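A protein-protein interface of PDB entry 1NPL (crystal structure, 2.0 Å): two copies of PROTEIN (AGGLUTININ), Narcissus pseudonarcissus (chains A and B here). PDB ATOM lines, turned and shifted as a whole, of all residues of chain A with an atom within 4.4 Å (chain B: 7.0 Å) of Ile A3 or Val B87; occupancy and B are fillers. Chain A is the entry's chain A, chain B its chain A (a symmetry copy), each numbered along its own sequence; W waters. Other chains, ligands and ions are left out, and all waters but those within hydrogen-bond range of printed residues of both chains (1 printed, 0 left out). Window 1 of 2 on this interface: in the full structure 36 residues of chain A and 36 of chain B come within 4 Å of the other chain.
O of Asn B2 is in hydrogen-bond range of N of Leu B88. The backbone NH (N) of Lys B90 lies close to the side-chain amide nitrogen (ND2) of Asn B18 (3.4 Å). The backbone carbonyl oxygen (O) of Val B85 sits at hydrogen-bond distance from the backbone NH (N) of Tyr B97, at 2.9 Å. The backbone NH (N) of Val B87 is in hydrogen-bond range of the backbone carbonyl oxygen (O) of Val B95, 2.9 Å away. The side-chain amide oxygen (OE1) of Gln B89 is in hydrogen-bond range of the side-chain hydroxyl (OH) of Tyr B97, 2.6 Å away.
Ile B3 touches Asn A2 (CD1 to ND2, 3.9 Å). ND2 of Asn B2 touches CD1 of Ile A3, 3.9 Å away. Ile B3 touches Ile A3. Val B87 touches Ile A3. Gln B89 touches Tyr A5. Lys B90 touches Tyr A5. CG1 of Val A85 touches CE1 of Tyr B97, at 3.7 Å. Ile B3 touches Val A87 (CD1 to CG1, 3.8 Å).
Hydrophobic or aromatic side chains of chain B within 4 Å of the printed part of chain A: Ile B3, Val B87 and Tyr B97. Printed residues of chain A that touch a printed residue of chain B: Asn A2, Ile A3, Tyr A5, Val A85 and Val A87. Hydrophobic or aromatic side chains of chain A within 4 Å of the printed part of chain B: Ile A3, Tyr A5, Val A85 and Val A87. Among the printed residues, 9 pairs touch across the chains. Among the printed residues, no Asp or Glu carboxylate lies within 4 Å of a Lys or Arg side-chain nitrogen of the other chain.
Water W1 lies within hydrogen-bond range of NZ of Lys B90 (2.7 Å), O of Ile A3 (3.2 Å) and OD1 of Asp A1 (3.4 Å).
Asn A2 touches its own counterpart, Asn B2. Asn A2 touches Ile B3, and with the chains exchanged Ile A3 touches Asn B2. Ile A3 touches its own counterpart, Ile B3. Ile A3 touches Val B87, and with the chains exchanged Val A87 touches Ile B3.
Ile A3 touches just these residues of chain B: Asn B2, Ile B3 and Val B87. Of the printed residues of chain B, Tyr A5 touches Gln B89 and Lys B90. Printed residues of chain A within 4 Å of Asn B2: Asn A2 and Ile A3. Of chain A, only Ile A3 comes within 4 Å of Val B87. Of the printed residues of chain A, Lys B90 touches Tyr A5. Val B94 touches none of the printed residues of chain A. Of the printed residues of chain A, Tyr B97 touches Val A85. The nearest printed residue of chain B that does not touch Asn A2 is Asn B18 (6.9 Å).
The side-chain amide oxygen of Asn A2 lies close to the side-chain amide oxygen of Asn B2, 3.5 Å away.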
ATOM      1  N   ASP A   1      32.991  11.033  29.661  1.00  0.00           N
ATOM      2  CA  ASP A   1      33.140  11.280  28.195  1.00  0.00           C
ATOM      3  C   ASP A   1      31.897  11.856  27.536  1.00  0.00           C
ATOM      4  O   ASP A   1      30.842  11.917  28.181  1.00  0.00           O
ATOM      5  CB  ASP A   1      33.571   9.984  27.534  1.00  0.00           C
ATOM      6  CG  ASP A   1      32.490   9.084  27.006  1.00  0.00           C
ATOM      7  OD1 ASP A   1      31.384   8.956  27.581  1.00  0.00           O
ATOM      8  OD2 ASP A   1      32.715   8.447  25.940  1.00  0.00           O
ATOM      9  N   ASN A   2      31.828  12.093  26.226  1.00  0.00           N
ATOM     10  CA  ASN A   2      30.978  13.119  25.683  1.00  0.00           C
ATOM     11  C   ASN A   2      29.484  12.814  25.755  1.00  0.00           C
ATOM     12  O   ASN A   2      28.743  13.606  25.138  1.00  0.00           O
ATOM     13  CB  ASN A   2      31.472  13.433  24.268  1.00  0.00           C
ATOM     14  CG  ASN A   2      31.332  12.320  23.246  1.00  0.00           C
ATOM     15  OD1 ASN A   2      31.309  11.143  23.512  1.00  0.00           O
ATOM     16  ND2 ASN A   2      31.245  12.646  21.951  1.00  0.00           N
ATOM     17  N   ILE A   3      29.064  11.712  26.355  1.00  0.00           N
ATOM     18  CA  ILE A   3      27.630  11.360  26.356  1.00  0.00           C
ATOM     19  C   ILE A   3      27.103  11.023  27.734  1.00  0.00           C
ATOM     20  O   ILE A   3      27.803  10.296  28.441  1.00  0.00           O
ATOM     21  CB  ILE A   3      27.399  10.110  25.453  1.00  0.00           C
ATOM     22  CG1 ILE A   3      27.931  10.485  24.048  1.00  0.00           C
ATOM     23  CG2 ILE A   3      25.944   9.678  25.354  1.00  0.00           C
ATOM     24  CD1 ILE A   3      27.698   9.505  22.940  1.00  0.00           C
ATOM     25  N   LEU A   4      25.921  11.530  28.110  1.00  0.00           N
ATOM     26  CA  LEU A   4      25.198  11.111  29.287  1.00  0.00           C
ATOM     27  C   LEU A   4      24.015  10.256  28.824  1.00  0.00           C
ATOM     28  O   LEU A   4      23.237  10.846  28.060  1.00  0.00           O
ATOM     29  CB  LEU A   4      24.699  12.337  30.103  1.00  0.00           C
ATOM     30  CG  LEU A   4      24.027  12.012  31.436  1.00  0.00           C
ATOM     31  CD1 LEU A   4      24.945  11.310  32.409  1.00  0.00           C
ATOM     32  CD2 LEU A   4      23.486  13.314  32.090  1.00  0.00           C
ATOM     33  N   TYR A   5      23.872   8.992  29.242  1.00  0.00           N
ATOM     34  CA  TYR A   5      22.815   8.149  28.677  1.00  0.00           C
ATOM     35  C   TYR A   5      21.547   8.299  29.541  1.00  0.00           C
ATOM     36  O   TYR A   5      21.700   8.581  30.741  1.00  0.00           O
ATOM     37  CB  TYR A   5      23.195   6.653  28.610  1.00  0.00           C
ATOM     38  CG  TYR A   5      24.261   6.376  27.528  1.00  0.00           C
ATOM     39  CD1 TYR A   5      25.605   6.547  27.878  1.00  0.00           C
ATOM     40  CD2 TYR A   5      23.929   6.023  26.231  1.00  0.00           C
ATOM     41  CE1 TYR A   5      26.624   6.323  26.949  1.00  0.00           C
ATOM     42  CE2 TYR A   5      24.940   5.806  25.300  1.00  0.00           C
ATOM     43  CZ  TYR A   5      26.255   5.942  25.638  1.00  0.00           C
ATOM     44  OH  TYR A   5      27.277   5.775  24.732  1.00  0.00           O
ATOM     45  N   LEU A  16      30.788  16.151  31.447  1.00  0.00           N
ATOM     46  CA  LEU A  16      31.162  15.704  30.109  1.00  0.00           C
ATOM     47  C   LEU A  16      32.259  16.534  29.461  1.00  0.00           C
ATOM     48  O   LEU A  16      32.404  17.702  29.799  1.00  0.00           O
ATOM     49  CB  LEU A  16      30.005  15.647  29.080  1.00  0.00           C
ATOM     50  CG  LEU A  16      28.684  15.051  29.631  1.00  0.00           C
ATOM     51  CD1 LEU A  16      27.608  15.277  28.591  1.00  0.00           C
ATOM     52  CD2 LEU A  16      28.887  13.605  30.112  1.00  0.00           C
ATOM     53  N   VAL A  85      19.909  10.101  24.646  1.00  0.00           N
ATOM     54  CA  VAL A  85      21.258  10.573  24.993  1.00  0.00           C
ATOM     55  C   VAL A  85      21.330  12.128  24.970  1.00  0.00           C
ATOM     56  O   VAL A  85      20.757  12.849  24.139  1.00  0.00           O
ATOM     57  CB  VAL A  85      22.351  10.059  24.020  1.00  0.00           C
ATOM     58  CG1 VAL A  85      22.453   8.539  24.056  1.00  0.00           C
ATOM     59  CG2 VAL A  85      22.045  10.421  22.545  1.00  0.00           C
ATOM     60  N   CYS A  86      22.043  12.672  25.937  1.00  0.00           N
ATOM     61  CA  CYS A  86      22.587  14.022  25.909  1.00  0.00           C
ATOM     62  C   CYS A  86      24.075  14.040  25.482  1.00  0.00           C
ATOM     63  O   CYS A  86      24.905  13.395  26.123  1.00  0.00           O
ATOM     64  CB  CYS A  86      22.396  14.621  27.294  1.00  0.00           C
ATOM     65  SG  CYS A  86      23.051  16.304  27.554  1.00  0.00           S
ATOM     66  N   VAL A  87      24.414  14.787  24.435  1.00  0.00           N
ATOM     67  CA  VAL A  87      25.690  14.717  23.760  1.00  0.00           C
ATOM     68  C   VAL A  87      26.383  16.101  23.838  1.00  0.00           C
ATOM     69  O   VAL A  87      25.735  17.072  23.417  1.00  0.00           O
ATOM     70  CB  VAL A  87      25.613  14.266  22.288  1.00  0.00           C
ATOM     71  CG1 VAL A  87      27.040  14.106  21.725  1.00  0.00           C
ATOM     72  CG2 VAL A  87      24.925  12.900  22.148  1.00  0.00           C
ATOM     73  N   ASN B   2      33.250   8.093  18.403  1.00  0.00           N
ATOM     74  CA  ASN B   2      32.175   7.150  18.553  1.00  0.00           C
ATOM     75  C   ASN B   2      30.857   7.574  17.909  1.00  0.00           C
ATOM     76  O   ASN B   2      29.873   6.855  18.175  1.00  0.00           O
ATOM     77  CB  ASN B   2      32.051   6.820  20.044  1.00  0.00           C
ATOM     78  CG  ASN B   2      31.614   7.957  20.949  1.00  0.00           C
ATOM     79  OD1 ASN B   2      31.793   9.128  20.714  1.00  0.00           O
ATOM     80  ND2 ASN B   2      31.002   7.660  22.101  1.00  0.00           N
ATOM     81  N   ILE B   3      30.797   8.696  17.211  1.00  0.00           N
ATOM     82  CA  ILE B   3      29.510   9.164  16.657  1.00  0.00           C
ATOM     83  C   ILE B   3      29.592   9.520  15.188  1.00  0.00           C
ATOM     84  O   ILE B   3      30.570  10.176  14.823  1.00  0.00           O
ATOM     85  CB  ILE B   3      29.048  10.444  17.419  1.00  0.00           C
ATOM     86  CG1 ILE B   3      28.958  10.049  18.914  1.00  0.00           C
ATOM     87  CG2 ILE B   3      27.710  10.995  16.949  1.00  0.00           C
ATOM     88  CD1 ILE B   3      28.392  11.064  19.859  1.00  0.00           C
ATOM     89  N   LEU B   4      28.614   9.105  14.373  1.00  0.00           N
ATOM     90  CA  LEU B   4      28.444   9.562  13.014  1.00  0.00           C
ATOM     91  C   LEU B   4      27.248  10.518  12.993  1.00  0.00           C
ATOM     92  O   LEU B   4      26.188  10.006  13.383  1.00  0.00           O
ATOM     93  CB  LEU B   4      28.205   8.367  12.048  1.00  0.00           C
ATOM     94  CG  LEU B   4      28.135   8.725  10.564  1.00  0.00           C
ATOM     95  CD1 LEU B   4      29.414   9.333  10.039  1.00  0.00           C
ATOM     96  CD2 LEU B   4      27.787   7.460   9.729  1.00  0.00           C
ATOM     97  N   LEU B  16      34.002   4.047  13.123  1.00  0.00           N
ATOM     98  CA  LEU B  16      33.859   4.485  14.508  1.00  0.00           C
ATOM     99  C   LEU B  16      34.546   3.578  15.519  1.00  0.00           C
ATOM    100  O   LEU B  16      34.714   2.397  15.245  1.00  0.00           O
ATOM    101  CB  LEU B  16      32.402   4.653  15.005  1.00  0.00           C
ATOM    102  CG  LEU B  16      31.454   5.346  13.992  1.00  0.00           C
ATOM    103  CD1 LEU B  16      30.043   5.226  14.526  1.00  0.00           C
ATOM    104  CD2 LEU B  16      31.946   6.762  13.653  1.00  0.00           C
ATOM    105  N   ASN B  18      35.199   2.761  19.946  1.00  0.00           N
ATOM    106  CA  ASN B  18      34.987   3.045  21.358  1.00  0.00           C
ATOM    107  C   ASN B  18      35.696   1.967  22.172  1.00  0.00           C
ATOM    108  O   ASN B  18      35.268   0.789  22.229  1.00  0.00           O
ATOM    109  CB  ASN B  18      33.437   3.042  21.594  1.00  0.00           C
ATOM    110  CG  ASN B  18      33.003   3.732  22.867  1.00  0.00           C
ATOM    111  OD1 ASN B  18      33.841   3.766  23.784  1.00  0.00           O
ATOM    112  ND2 ASN B  18      31.768   4.315  23.023  1.00  0.00           N
ATOM    113  N   PHE B  23      33.711  -0.117  14.503  1.00  0.00           N
ATOM    114  CA  PHE B  23      32.618  -0.333  13.507  1.00  0.00           C
ATOM    115  C   PHE B  23      33.048   0.272  12.195  1.00  0.00           C
ATOM    116  O   PHE B  23      33.193   1.518  12.030  1.00  0.00           O
ATOM    117  CB  PHE B  23      31.367   0.365  14.062  1.00  0.00           C
ATOM    118  CG  PHE B  23      30.065   0.255  13.331  1.00  0.00           C
ATOM    119  CD1 PHE B  23      29.443  -0.976  13.179  1.00  0.00           C
ATOM    120  CD2 PHE B  23      29.440   1.399  12.845  1.00  0.00           C
ATOM    121  CE1 PHE B  23      28.173  -1.056  12.546  1.00  0.00           C
ATOM    122  CE2 PHE B  23      28.180   1.308  12.201  1.00  0.00           C
ATOM    123  CZ  PHE B  23      27.583   0.102  12.080  1.00  0.00           C
ATOM    124  N   VAL B  85      21.865  11.077  15.240  1.00  0.00           N
ATOM    125  CA  VAL B  85      23.199  10.491  15.439  1.00  0.00           C
ATOM    126  C   VAL B  85      23.129   8.936  15.462  1.00  0.00           C
ATOM    127  O   VAL B  85      22.220   8.278  15.992  1.00  0.00           O
ATOM    128  CB  VAL B  85      23.864  10.931  16.770  1.00  0.00           C
ATOM    129  CG1 VAL B  85      24.095  12.436  16.802  1.00  0.00           C
ATOM    130  CG2 VAL B  85      22.978  10.619  18.002  1.00  0.00           C
ATOM    131  N   CYS B  86      24.116   8.319  14.841  1.00  0.00           N
ATOM    132  CA  CYS B  86      24.494   6.931  15.057  1.00  0.00           C
ATOM    133  C   CYS B  86      25.690   6.798  16.031  1.00  0.00           C
ATOM    134  O   CYS B  86      26.754   7.363  15.775  1.00  0.00           O
ATOM    135  CB  CYS B  86      24.810   6.326  13.698  1.00  0.00           C
ATOM    136  SG  CYS B  86      25.375   4.591  13.685  1.00  0.00           S
ATOM    137  N   VAL B  87      25.532   6.043  17.114  1.00  0.00           N
ATOM    138  CA  VAL B  87      26.445   6.020  18.234  1.00  0.00           C
ATOM    139  C   VAL B  87      26.997   4.583  18.410  1.00  0.00           C
ATOM    140  O   VAL B  87      26.159   3.676  18.528  1.00  0.00           O
ATOM    141  CB  VAL B  87      25.836   6.500  19.567  1.00  0.00           C
ATOM    142  CG1 VAL B  87      26.938   6.553  20.645  1.00  0.00           C
ATOM    143  CG2 VAL B  87      25.262   7.921  19.450  1.00  0.00           C
ATOM    144  N   LEU B  88      28.307   4.437  18.464  1.00  0.00           N
ATOM    145  CA  LEU B  88      28.870   3.155  18.985  1.00  0.00           C
ATOM    146  C   LEU B  88      29.000   3.269  20.470  1.00  0.00           C
ATOM    147  O   LEU B  88      29.911   4.026  20.894  1.00  0.00           O
ATOM    148  CB  LEU B  88      30.309   2.980  18.396  1.00  0.00           C
ATOM    149  CG  LEU B  88      30.874   1.551  18.234  1.00  0.00           C
ATOM    150  CD1 LEU B  88      32.395   1.613  17.976  1.00  0.00           C
ATOM    151  CD2 LEU B  88      30.442   0.503  19.249  1.00  0.00           C
ATOM    152  N   GLN B  89      28.221   2.621  21.301  1.00  0.00           N
ATOM    153  CA  GLN B  89      28.163   2.937  22.727  1.00  0.00           C
ATOM    154  C   GLN B  89      29.177   2.137  23.544  1.00  0.00           C
ATOM    155  O   GLN B  89      29.682   1.133  23.053  1.00  0.00           O
ATOM    156  CB  GLN B  89      26.737   2.666  23.306  1.00  0.00           C
ATOM    157  CG  GLN B  89      25.638   3.293  22.423  1.00  0.00           C
ATOM    158  CD  GLN B  89      24.246   3.232  23.093  1.00  0.00           C
ATOM    159  OE1 GLN B  89      23.429   4.104  22.820  1.00  0.00           O
ATOM    160  NE2 GLN B  89      23.919   2.263  23.944  1.00  0.00           N
ATOM    161  N   LYS B  90      29.365   2.615  24.755  1.00  0.00           N
ATOM    162  CA  LYS B  90      30.234   1.969  25.727  1.00  0.00           C
ATOM    163  C   LYS B  90      29.786   0.565  26.123  1.00  0.00           C
ATOM    164  O   LYS B  90      30.623  -0.305  26.334  1.00  0.00           O
ATOM    165  CB  LYS B  90      30.370   2.910  26.934  1.00  0.00           C
ATOM    166  CG  LYS B  90      29.043   2.993  27.747  1.00  0.00           C
ATOM    167  CD  LYS B  90      29.358   3.759  29.053  1.00  0.00           C
ATOM    168  CE  LYS B  90      28.025   3.984  29.814  1.00  0.00           C
ATOM    169  NZ  LYS B  90      28.127   5.231  30.653  1.00  0.00           N
ATOM    170  N   ASN B  93      26.494  -1.645  22.141  1.00  0.00           N
ATOM    171  CA  ASN B  93      25.420  -1.578  21.112  1.00  0.00           C
ATOM    172  C   ASN B  93      25.722  -0.476  20.105  1.00  0.00           C
ATOM    173  O   ASN B  93      26.378   0.523  20.460  1.00  0.00           O
ATOM    174  CB  ASN B  93      24.119  -1.191  21.866  1.00  0.00           C
ATOM    175  CG  ASN B  93      22.900  -1.889  21.292  1.00  0.00           C
ATOM    176  OD1 ASN B  93      22.919  -2.425  20.182  1.00  0.00           O
ATOM    177  ND2 ASN B  93      21.848  -1.798  22.096  1.00  0.00           N
ATOM    178  N   VAL B  94      25.259  -0.533  18.874  1.00  0.00           N
ATOM    179  CA  VAL B  94      25.297   0.566  17.935  1.00  0.00           C
ATOM    180  C   VAL B  94      23.839   1.012  17.744  1.00  0.00           C
ATOM    181  O   VAL B  94      22.999   0.158  17.476  1.00  0.00           O
ATOM    182  CB  VAL B  94      25.888   0.165  16.554  1.00  0.00           C
ATOM    183  CG1 VAL B  94      25.930   1.317  15.572  1.00  0.00           C
ATOM    184  CG2 VAL B  94      27.356  -0.328  16.792  1.00  0.00           C
ATOM    185  N   VAL B  95      23.600   2.316  17.968  1.00  0.00           N
ATOM    186  CA  VAL B  95      22.186   2.736  18.135  1.00  0.00           C
ATOM    187  C   VAL B  95      21.959   4.029  17.349  1.00  0.00           C
ATOM    188  O   VAL B  95      22.831   4.948  17.417  1.00  0.00           O
ATOM    189  CB  VAL B  95      21.891   2.892  19.640  1.00  0.00           C
ATOM    190  CG1 VAL B  95      20.429   3.353  19.857  1.00  0.00           C
ATOM    191  CG2 VAL B  95      22.159   1.669  20.503  1.00  0.00           C
ATOM    192  N   ILE B  96      20.871   4.153  16.608  1.00  0.00           N
ATOM    193  CA  ILE B  96      20.480   5.437  15.993  1.00  0.00           C
ATOM    194  C   ILE B  96      19.471   6.162  16.878  1.00  0.00           C
ATOM    195  O   ILE B  96      18.403   5.583  17.240  1.00  0.00           O
ATOM    196  CB  ILE B  96      19.890   5.298  14.569  1.00  0.00           C
ATOM    197  CG1 ILE B  96      20.877   4.680  13.553  1.00  0.00           C
ATOM    198  CG2 ILE B  96      19.407   6.626  13.964  1.00  0.00           C
ATOM    199  CD1 ILE B  96      20.104   4.112  12.358  1.00  0.00           C
ATOM    200  N   TYR B  97      19.744   7.450  17.162  1.00  0.00           N
ATOM    201  CA  TYR B  97      18.871   8.285  17.974  1.00  0.00           C
ATOM    202  C   TYR B  97      18.443   9.557  17.190  1.00  0.00           C
ATOM    203  O   TYR B  97      19.233  10.266  16.535  1.00  0.00           O
ATOM    204  CB  TYR B  97      19.428   8.820  19.327  1.00  0.00           C
ATOM    205  CG  TYR B  97      19.844   7.793  20.366  1.00  0.00           C
ATOM    206  CD1 TYR B  97      21.151   7.256  20.349  1.00  0.00           C
ATOM    207  CD2 TYR B  97      18.990   7.338  21.357  1.00  0.00           C
ATOM    208  CE1 TYR B  97      21.566   6.327  21.284  1.00  0.00           C
ATOM    209  CE2 TYR B  97      19.376   6.414  22.288  1.00  0.00           C
ATOM    210  CZ  TYR B  97      20.649   5.896  22.244  1.00  0.00           C
ATOM    211  OH  TYR B  97      21.009   4.991  23.226  1.00  0.00           O
HETATM  212  O   HOH W   1      28.928   7.489  29.482  1.00  0.00           O
